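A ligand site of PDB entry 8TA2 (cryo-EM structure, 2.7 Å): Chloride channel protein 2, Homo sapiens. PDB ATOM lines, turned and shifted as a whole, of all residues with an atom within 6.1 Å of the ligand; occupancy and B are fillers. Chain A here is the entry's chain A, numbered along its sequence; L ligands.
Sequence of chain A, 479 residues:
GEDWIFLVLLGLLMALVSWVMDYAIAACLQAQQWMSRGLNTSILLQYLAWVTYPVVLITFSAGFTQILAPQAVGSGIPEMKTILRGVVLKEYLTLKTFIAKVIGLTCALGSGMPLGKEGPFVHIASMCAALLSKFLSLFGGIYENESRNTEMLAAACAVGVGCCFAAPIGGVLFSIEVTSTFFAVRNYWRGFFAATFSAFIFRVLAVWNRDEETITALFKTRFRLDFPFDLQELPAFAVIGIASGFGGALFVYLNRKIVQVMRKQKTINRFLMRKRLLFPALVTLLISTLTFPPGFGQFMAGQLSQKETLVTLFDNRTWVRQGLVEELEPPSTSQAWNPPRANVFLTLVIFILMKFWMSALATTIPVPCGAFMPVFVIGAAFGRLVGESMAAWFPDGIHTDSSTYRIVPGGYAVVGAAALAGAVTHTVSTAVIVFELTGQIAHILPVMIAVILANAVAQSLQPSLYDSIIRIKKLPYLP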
ATOM      1  N   MET A  21      34.010 -15.816 -23.099  1.00  0.00           N
ATOM      2  CA  MET A  21      32.920 -16.218 -23.984  1.00  0.00           C
ATOM      3  C   MET A  21      32.056 -17.337 -23.401  1.00  0.00           C
ATOM      4  O   MET A  21      30.842 -17.276 -23.520  1.00  0.00           O
ATOM      5  CB  MET A  21      33.474 -16.644 -25.348  1.00  0.00           C
ATOM      6  CG  MET A  21      34.046 -15.450 -26.098  1.00  0.00           C
ATOM      7  SD  MET A  21      34.847 -15.895 -27.653  1.00  0.00           S
ATOM      8  CE  MET A  21      33.383 -16.297 -28.616  1.00  0.00           C
ATOM      9  N   ASP A  22      32.643 -18.340 -22.756  1.00  0.00           N
ATOM     10  CA  ASP A  22      31.875 -19.427 -22.130  1.00  0.00           C
ATOM     11  C   ASP A  22      31.069 -18.951 -20.911  1.00  0.00           C
ATOM     12  O   ASP A  22      29.992 -19.459 -20.635  1.00  0.00           O
ATOM     13  CB  ASP A  22      32.797 -20.581 -21.748  1.00  0.00           C
ATOM     14  CG  ASP A  22      33.181 -21.512 -22.912  1.00  0.00           C
ATOM     15  OD1 ASP A  22      32.897 -21.214 -24.096  1.00  0.00           O
ATOM     16  OD2 ASP A  22      33.697 -22.612 -22.635  1.00  0.00           O
ATOM     17  N   TYR A  23      31.542 -17.906 -20.219  1.00  0.00           N
ATOM     18  CA  TYR A  23      30.774 -17.228 -19.183  1.00  0.00           C
ATOM     19  C   TYR A  23      29.525 -16.543 -19.771  1.00  0.00           C
ATOM     20  O   TYR A  23      28.410 -16.773 -19.311  1.00  0.00           O
ATOM     21  CB  TYR A  23      31.690 -16.241 -18.461  1.00  0.00           C
ATOM     22  CG  TYR A  23      30.995 -15.455 -17.375  1.00  0.00           C
ATOM     23  CD1 TYR A  23      30.746 -16.056 -16.122  1.00  0.00           C
ATOM     24  CD2 TYR A  23      30.558 -14.133 -17.619  1.00  0.00           C
ATOM     25  CE1 TYR A  23      30.032 -15.350 -15.142  1.00  0.00           C
ATOM     26  CE2 TYR A  23      29.852 -13.433 -16.637  1.00  0.00           C
ATOM     27  CZ  TYR A  23      29.577 -14.041 -15.393  1.00  0.00           C
ATOM     28  OH  TYR A  23      28.884 -13.369 -14.448  1.00  0.00           O
ATOM     29  N   ILE A  25      28.012 -17.121 -22.786  1.00  0.00           N
ATOM     30  CA  ILE A  25      27.088 -18.126 -23.348  1.00  0.00           C
ATOM     31  C   ILE A  25      26.270 -18.787 -22.244  1.00  0.00           C
ATOM     32  O   ILE A  25      25.053 -18.905 -22.387  1.00  0.00           O
ATOM     33  CB  ILE A  25      27.864 -19.156 -24.202  1.00  0.00           C
ATOM     34  CG1 ILE A  25      28.381 -18.474 -25.487  1.00  0.00           C
ATOM     35  CG2 ILE A  25      26.996 -20.365 -24.577  1.00  0.00           C
ATOM     36  CD1 ILE A  25      29.512 -19.228 -26.175  1.00  0.00           C
ATOM     37  N   ALA A  26      26.887 -19.170 -21.118  1.00  0.00           N
ATOM     38  CA  ALA A  26      26.176 -19.773 -19.989  1.00  0.00           C
ATOM     39  C   ALA A  26      25.137 -18.812 -19.378  1.00  0.00           C
ATOM     40  O   ALA A  26      24.017 -19.225 -19.121  1.00  0.00           O
ATOM     41  CB  ALA A  26      27.185 -20.212 -18.932  1.00  0.00           C
ATOM     42  N   LEU A  29      22.053 -18.767 -21.707  1.00  0.00           N
ATOM     43  CA  LEU A  29      21.300 -20.017 -21.544  1.00  0.00           C
ATOM     44  C   LEU A  29      20.591 -20.118 -20.179  1.00  0.00           C
ATOM     45  O   LEU A  29      19.533 -20.729 -20.081  1.00  0.00           O
ATOM     46  CB  LEU A  29      22.264 -21.197 -21.736  1.00  0.00           C
ATOM     47  CG  LEU A  29      22.734 -21.393 -23.193  1.00  0.00           C
ATOM     48  CD1 LEU A  29      23.978 -22.263 -23.218  1.00  0.00           C
ATOM     49  CD2 LEU A  29      21.665 -22.079 -24.034  1.00  0.00           C
ATOM     50  N   LEU A 109      25.364 -18.962 -30.039  1.00  0.00           N
ATOM     51  CA  LEU A 109      25.423 -20.083 -29.105  1.00  0.00           C
ATOM     52  C   LEU A 109      24.601 -19.866 -27.821  1.00  0.00           C
ATOM     53  O   LEU A 109      24.089 -20.833 -27.278  1.00  0.00           O
ATOM     54  CB  LEU A 109      26.884 -20.373 -28.745  1.00  0.00           C
ATOM     55  CG  LEU A 109      27.759 -20.841 -29.915  1.00  0.00           C
ATOM     56  CD1 LEU A 109      29.182 -21.001 -29.427  1.00  0.00           C
ATOM     57  CD2 LEU A 109      27.320 -22.184 -30.494  1.00  0.00           C
ATOM     58  N   MET A 113      20.185 -23.109 -30.640  1.00  0.00           N
ATOM     59  CA  MET A 113      20.501 -23.530 -32.016  1.00  0.00           C
ATOM     60  C   MET A 113      21.613 -24.597 -32.093  1.00  0.00           C
ATOM     61  O   MET A 113      22.620 -24.452 -31.388  1.00  0.00           O
ATOM     62  CB  MET A 113      20.871 -22.310 -32.879  1.00  0.00           C
ATOM     63  CG  MET A 113      19.683 -21.368 -33.124  1.00  0.00           C
ATOM     64  SD  MET A 113      18.236 -22.127 -33.904  1.00  0.00           S
ATOM     65  CE  MET A 113      17.164 -22.422 -32.466  1.00  0.00           C
ATOM     66  N   LEU A 115      24.595 -25.433 -33.148  1.00  0.00           N
ATOM     67  CA  LEU A 115      25.809 -24.821 -33.689  1.00  0.00           C
ATOM     68  C   LEU A 115      27.027 -25.238 -32.863  1.00  0.00           C
ATOM     69  O   LEU A 115      26.891 -25.604 -31.696  1.00  0.00           O
ATOM     70  CB  LEU A 115      25.625 -23.297 -33.746  1.00  0.00           C
ATOM     71  CG  LEU A 115      24.386 -22.786 -34.523  1.00  0.00           C
ATOM     72  CD1 LEU A 115      24.292 -21.272 -34.461  1.00  0.00           C
ATOM     73  CD2 LEU A 115      24.379 -23.191 -35.989  1.00  0.00           C
ATOM     74  N   GLY A 116      28.225 -25.234 -33.446  1.00  0.00           N
ATOM     75  CA  GLY A 116      29.501 -25.460 -32.757  1.00  0.00           C
ATOM     76  C   GLY A 116      30.399 -24.228 -32.742  1.00  0.00           C
ATOM     77  O   GLY A 116      30.042 -23.195 -33.286  1.00  0.00           O
ATOM     78  N   LYS A 117      31.606 -24.339 -32.171  1.00  0.00           N
ATOM     79  CA  LYS A 117      32.631 -23.294 -32.128  1.00  0.00           C
ATOM     80  C   LYS A 117      34.042 -23.716 -32.581  1.00  0.00           C
ATOM     81  O   LYS A 117      34.906 -22.856 -32.587  1.00  0.00           O
ATOM     82  CB  LYS A 117      32.630 -22.598 -30.749  1.00  0.00           C
ATOM     83  CG  LYS A 117      33.080 -23.454 -29.565  1.00  0.00           C
ATOM     84  CD  LYS A 117      32.609 -22.854 -28.225  1.00  0.00           C
ATOM     85  CE  LYS A 117      33.105 -23.726 -27.077  1.00  0.00           C
ATOM     86  NZ  LYS A 117      32.482 -23.351 -25.779  1.00  0.00           N
ATOM     87  N   CYS A 164      39.206 -24.832 -27.600  1.00  0.00           N
ATOM     88  CA  CYS A 164      37.838 -25.227 -27.900  1.00  0.00           C
ATOM     89  C   CYS A 164      37.443 -26.496 -27.126  1.00  0.00           C
ATOM     90  O   CYS A 164      36.543 -26.471 -26.304  1.00  0.00           O
ATOM     91  CB  CYS A 164      37.713 -25.401 -29.413  1.00  0.00           C
ATOM     92  SG  CYS A 164      36.010 -25.824 -29.826  1.00  0.00           S
ATOM     93  N   PHE A 165      38.162 -27.598 -27.357  1.00  0.00           N
ATOM     94  CA  PHE A 165      37.837 -28.895 -26.772  1.00  0.00           C
ATOM     95  C   PHE A 165      38.323 -29.081 -25.330  1.00  0.00           C
ATOM     96  O   PHE A 165      37.894 -30.009 -24.653  1.00  0.00           O
ATOM     97  CB  PHE A 165      38.420 -29.994 -27.674  1.00  0.00           C
ATOM     98  CG  PHE A 165      37.920 -30.028 -29.106  1.00  0.00           C
ATOM     99  CD1 PHE A 165      36.580 -29.741 -29.416  1.00  0.00           C
ATOM    100  CD2 PHE A 165      38.800 -30.405 -30.130  1.00  0.00           C
ATOM    101  CE1 PHE A 165      36.139 -29.783 -30.748  1.00  0.00           C
ATOM    102  CE2 PHE A 165      38.352 -30.475 -31.459  1.00  0.00           C
ATOM    103  CZ  PHE A 165      37.027 -30.148 -31.773  1.00  0.00           C
ATOM    104  N   PHE A 219      33.825 -32.890 -19.099  1.00  0.00           N
ATOM    105  CA  PHE A 219      33.014 -34.075 -19.435  1.00  0.00           C
ATOM    106  C   PHE A 219      33.554 -35.393 -18.864  1.00  0.00           C
ATOM    107  O   PHE A 219      33.343 -36.462 -19.429  1.00  0.00           O
ATOM    108  CB  PHE A 219      32.799 -34.129 -20.955  1.00  0.00           C
ATOM    109  CG  PHE A 219      32.126 -32.900 -21.521  1.00  0.00           C
ATOM    110  CD1 PHE A 219      30.729 -32.800 -21.515  1.00  0.00           C
ATOM    111  CD2 PHE A 219      32.891 -31.826 -22.008  1.00  0.00           C
ATOM    112  CE1 PHE A 219      30.102 -31.639 -22.001  1.00  0.00           C
ATOM    113  CE2 PHE A 219      32.263 -30.664 -22.481  1.00  0.00           C
ATOM    114  CZ  PHE A 219      30.873 -30.579 -22.493  1.00  0.00           C
ATOM    115  N   SER A 305      20.422 -27.925 -22.650  1.00  0.00           N
ATOM    116  CA  SER A 305      21.427 -27.343 -23.563  1.00  0.00           C
ATOM    117  C   SER A 305      22.277 -28.428 -24.242  1.00  0.00           C
ATOM    118  O   SER A 305      22.116 -29.618 -23.985  1.00  0.00           O
ATOM    119  CB  SER A 305      22.310 -26.358 -22.808  1.00  0.00           C
ATOM    120  OG  SER A 305      23.268 -27.039 -22.038  1.00  0.00           O
ATOM    121  N   GLN A 306      23.222 -28.050 -25.110  1.00  0.00           N
ATOM    122  CA  GLN A 306      24.136 -29.005 -25.743  1.00  0.00           C
ATOM    123  C   GLN A 306      25.094 -29.643 -24.728  1.00  0.00           C
ATOM    124  O   GLN A 306      25.209 -30.872 -24.685  1.00  0.00           O
ATOM    125  CB  GLN A 306      24.921 -28.350 -26.886  1.00  0.00           C
ATOM    126  CG  GLN A 306      24.020 -27.888 -28.035  1.00  0.00           C
ATOM    127  CD  GLN A 306      24.778 -27.714 -29.347  1.00  0.00           C
ATOM    128  OE1 GLN A 306      24.638 -28.479 -30.279  1.00  0.00           O
ATOM    129  NE2 GLN A 306      25.620 -26.717 -29.455  1.00  0.00           N
ATOM    130  N   LYS A 307      25.716 -28.865 -23.843  1.00  0.00           N
ATOM    131  CA  LYS A 307      26.539 -29.362 -22.727  1.00  0.00           C
ATOM    132  C   LYS A 307      25.731 -30.247 -21.790  1.00  0.00           C
ATOM    133  O   LYS A 307      26.179 -31.339 -21.457  1.00  0.00           O
ATOM    134  CB  LYS A 307      27.138 -28.168 -21.992  1.00  0.00           C
ATOM    135  CG  LYS A 307      28.036 -28.549 -20.806  1.00  0.00           C
ATOM    136  CD  LYS A 307      28.612 -27.324 -20.093  1.00  0.00           C
ATOM    137  CE  LYS A 307      29.693 -26.616 -20.915  1.00  0.00           C
ATOM    138  NZ  LYS A 307      30.259 -25.444 -20.202  1.00  0.00           N
ATOM    139  N   GLU A 308      24.531 -29.850 -21.381  1.00  0.00           N
ATOM    140  CA  GLU A 308      23.685 -30.662 -20.503  1.00  0.00           C
ATOM    141  C   GLU A 308      23.262 -31.969 -21.158  1.00  0.00           C
ATOM    142  O   GLU A 308      23.318 -33.024 -20.522  1.00  0.00           O
ATOM    143  CB  GLU A 308      22.448 -29.864 -20.099  1.00  0.00           C
ATOM    144  CG  GLU A 308      22.786 -28.663 -19.201  1.00  0.00           C
ATOM    145  CD  GLU A 308      21.670 -27.618 -19.115  1.00  0.00           C
ATOM    146  OE1 GLU A 308      20.611 -27.784 -19.758  1.00  0.00           O
ATOM    147  OE2 GLU A 308      21.857 -26.625 -18.383  1.00  0.00           O
ATOM    148  N   LEU A 310      25.066 -33.615 -23.559  1.00  0.00           N
ATOM    149  CA  LEU A 310      26.260 -34.457 -23.666  1.00  0.00           C
ATOM    150  C   LEU A 310      26.660 -35.079 -22.321  1.00  0.00           C
ATOM    151  O   LEU A 310      26.923 -36.279 -22.259  1.00  0.00           O
ATOM    152  CB  LEU A 310      27.388 -33.639 -24.305  1.00  0.00           C
ATOM    153  CG  LEU A 310      28.652 -34.450 -24.646  1.00  0.00           C
ATOM    154  CD1 LEU A 310      28.387 -35.573 -25.647  1.00  0.00           C
ATOM    155  CD2 LEU A 310      29.686 -33.509 -25.263  1.00  0.00           C
ATOM    156  N   PHE A 372      31.342 -28.995 -35.150  1.00  0.00           N
ATOM    157  CA  PHE A 372      31.805 -30.211 -34.466  1.00  0.00           C
ATOM    158  C   PHE A 372      30.868 -30.712 -33.334  1.00  0.00           C
ATOM    159  O   PHE A 372      30.447 -31.859 -33.379  1.00  0.00           O
ATOM    160  CB  PHE A 372      33.273 -30.046 -34.035  1.00  0.00           C
ATOM    161  CG  PHE A 372      33.955 -31.292 -33.501  1.00  0.00           C
ATOM    162  CD1 PHE A 372      33.738 -31.712 -32.177  1.00  0.00           C
ATOM    163  CD2 PHE A 372      34.867 -31.992 -34.309  1.00  0.00           C
ATOM    164  CE1 PHE A 372      34.409 -32.832 -31.663  1.00  0.00           C
ATOM    165  CE2 PHE A 372      35.555 -33.106 -33.794  1.00  0.00           C
ATOM    166  CZ  PHE A 372      35.327 -33.527 -32.478  1.00  0.00           C
ATOM    167  N   MET A 373      30.483 -29.879 -32.357  1.00  0.00           N
ATOM    168  CA  MET A 373      29.567 -30.269 -31.260  1.00  0.00           C
ATOM    169  C   MET A 373      28.239 -30.849 -31.751  1.00  0.00           C
ATOM    170  O   MET A 373      27.832 -31.889 -31.242  1.00  0.00           O
ATOM    171  CB  MET A 373      29.370 -29.108 -30.259  1.00  0.00           C
ATOM    172  CG  MET A 373      28.214 -29.265 -29.260  1.00  0.00           C
ATOM    173  SD  MET A 373      28.391 -30.518 -27.971  1.00  0.00           S
ATOM    174  CE  MET A 373      29.292 -29.571 -26.727  1.00  0.00           C
ATOM    175  N   PHE A 376      29.185 -34.429 -32.931  1.00  0.00           N
ATOM    176  CA  PHE A 376      29.648 -35.156 -31.750  1.00  0.00           C
ATOM    177  C   PHE A 376      28.480 -35.649 -30.883  1.00  0.00           C
ATOM    178  O   PHE A 376      28.446 -36.804 -30.480  1.00  0.00           O
ATOM    179  CB  PHE A 376      30.615 -34.245 -30.990  1.00  0.00           C
ATOM    180  CG  PHE A 376      31.444 -34.939 -29.944  1.00  0.00           C
ATOM    181  CD1 PHE A 376      32.688 -35.506 -30.288  1.00  0.00           C
ATOM    182  CD2 PHE A 376      30.968 -35.073 -28.627  1.00  0.00           C
ATOM    183  CE1 PHE A 376      33.460 -36.184 -29.324  1.00  0.00           C
ATOM    184  CE2 PHE A 376      31.745 -35.746 -27.670  1.00  0.00           C
ATOM    185  CZ  PHE A 376      32.980 -36.308 -28.015  1.00  0.00           C
ATOM    186  N   LEU A 437      39.006 -35.395 -22.996  1.00  0.00           N
ATOM    187  CA  LEU A 437      37.661 -35.001 -22.545  1.00  0.00           C
ATOM    188  C   LEU A 437      37.154 -35.906 -21.428  1.00  0.00           C
ATOM    189  O   LEU A 437      36.745 -35.436 -20.378  1.00  0.00           O
ATOM    190  CB  LEU A 437      36.647 -35.078 -23.700  1.00  0.00           C
ATOM    191  CG  LEU A 437      36.303 -33.726 -24.340  1.00  0.00           C
ATOM    192  CD1 LEU A 437      37.517 -33.070 -24.974  1.00  0.00           C
ATOM    193  CD2 LEU A 437      35.258 -33.957 -25.425  1.00  0.00           C
HETATM  194  C1  LIG L   1      30.658 -26.192 -28.073  1.00  0.00           C
HETATM  195  C2  LIG L   1      33.038 -29.892 -26.094  1.00  0.00           C
HETATM  196  C3  LIG L   1      32.783 -31.262 -26.016  1.00  0.00           C
HETATM  197  C4  LIG L   1      32.460 -31.986 -27.162  1.00  0.00           C
HETATM  198  C5  LIG L   1      32.674 -29.974 -28.490  1.00  0.00           C
HETATM  199  C6  LIG L   1      25.876 -25.301 -22.938  1.00  0.00           C
HETATM  200  C7  LIG L   1      27.111 -24.475 -22.904  1.00  0.00           C
HETATM  201  C8  LIG L   1      27.329 -23.586 -21.895  1.00  0.00           C
HETATM  202  C9  LIG L   1      28.432 -22.795 -21.928  1.00  0.00           C
HETATM  203  C10 LIG L   1      29.326 -22.934 -22.963  1.00  0.00           C
HETATM  204  C11 LIG L   1      28.091 -24.573 -23.871  1.00  0.00           C
HETATM  205  C12 LIG L   1      28.878 -25.772 -25.943  1.00  0.00           C
HETATM  206  C13 LIG L   1      28.519 -25.404 -27.239  1.00  0.00           C
HETATM  207  C14 LIG L   1      29.394 -25.618 -28.308  1.00  0.00           C
HETATM  208  C15 LIG L   1      31.031 -26.595 -26.778  1.00  0.00           C
HETATM  209  C16 LIG L   1      33.188 -27.732 -27.408  1.00  0.00           C
HETATM  210  C17 LIG L   1      32.971 -29.231 -27.335  1.00  0.00           C
HETATM  211  C18 LIG L   1      32.414 -31.349 -28.404  1.00  0.00           C
HETATM  212  C19 LIG L   1      30.128 -26.388 -25.717  1.00  0.00           C
HETATM  213  N1  LIG L   1      29.146 -23.818 -23.904  1.00  0.00           N
HETATM  214  N2  LIG L   1      28.022 -25.478 -24.889  1.00  0.00           N
HETATM  215  O1  LIG L   1      25.631 -25.997 -23.906  1.00  0.00           O
HETATM  216  O2  LIG L   1      25.164 -25.289 -21.949  1.00  0.00           O
HETATM  217  O3  LIG L   1      32.292 -27.061 -26.486  1.00  0.00           O
HETATM  218 CL1  LIG L   1      26.987 -24.592 -27.532  1.00  0.00          CL
HETATM  219 CL2  LIG L   1      30.535 -26.972 -24.111  1.00  0.00          CL
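O of Asp 22 touches C9 of the ligand, 3.9 Å away. Ile 25 touches the ligand (CG2 to C10, 3.8 Å). Leu 29 touches the ligand. Leu 109 touches the ligand (CD2 to CL1, 3.8 Å). Lys 117 touches the ligand (CE to O3, 3.5 Å). Cys 164 touches the ligand (O to C16, 3.8 Å). CE2 of Phe 219 touches C3 of the ligand (3.6 Å). Leu 310 touches the ligand (CD2 to C4, 3.7 Å). CE of Met 373 touches C19 of the ligand, at 3.4 Å. Phe 376 touches the ligand (CD2 to C4, 3.7 Å). Leu 437 touches the ligand. Within 4 Å of the ligand: Asp 22, Ile 25, Leu 29, Leu 109, Lys 117, Cys 164, Phe 219, Ser 305, Gln 306, Lys 307, Leu 310, Met 373, Phe 376 and Leu 437.
O2 of the ligand is in hydrogen-bond range of OG of Ser 305. N of Lys 307 lies within hydrogen-bond range of O1 of the ligand. N of Gln 306 lies within hydrogen-bond range of O1 of the ligand (3.4 Å).
The backbone NH of Ser 305 is in hydrogen-bond range of the side-chain carboxylate of Glu 308, at 2.9 Å. NE2 of Gln 306 sits at hydrogen-bond distance from O of Leu 115 (2.8 Å). The side-chain carboxylate (OD1) of Asp 22 is in salt-bridge range of the side-chain amino group (NZ) of Lys 117, 2.8 Å away.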
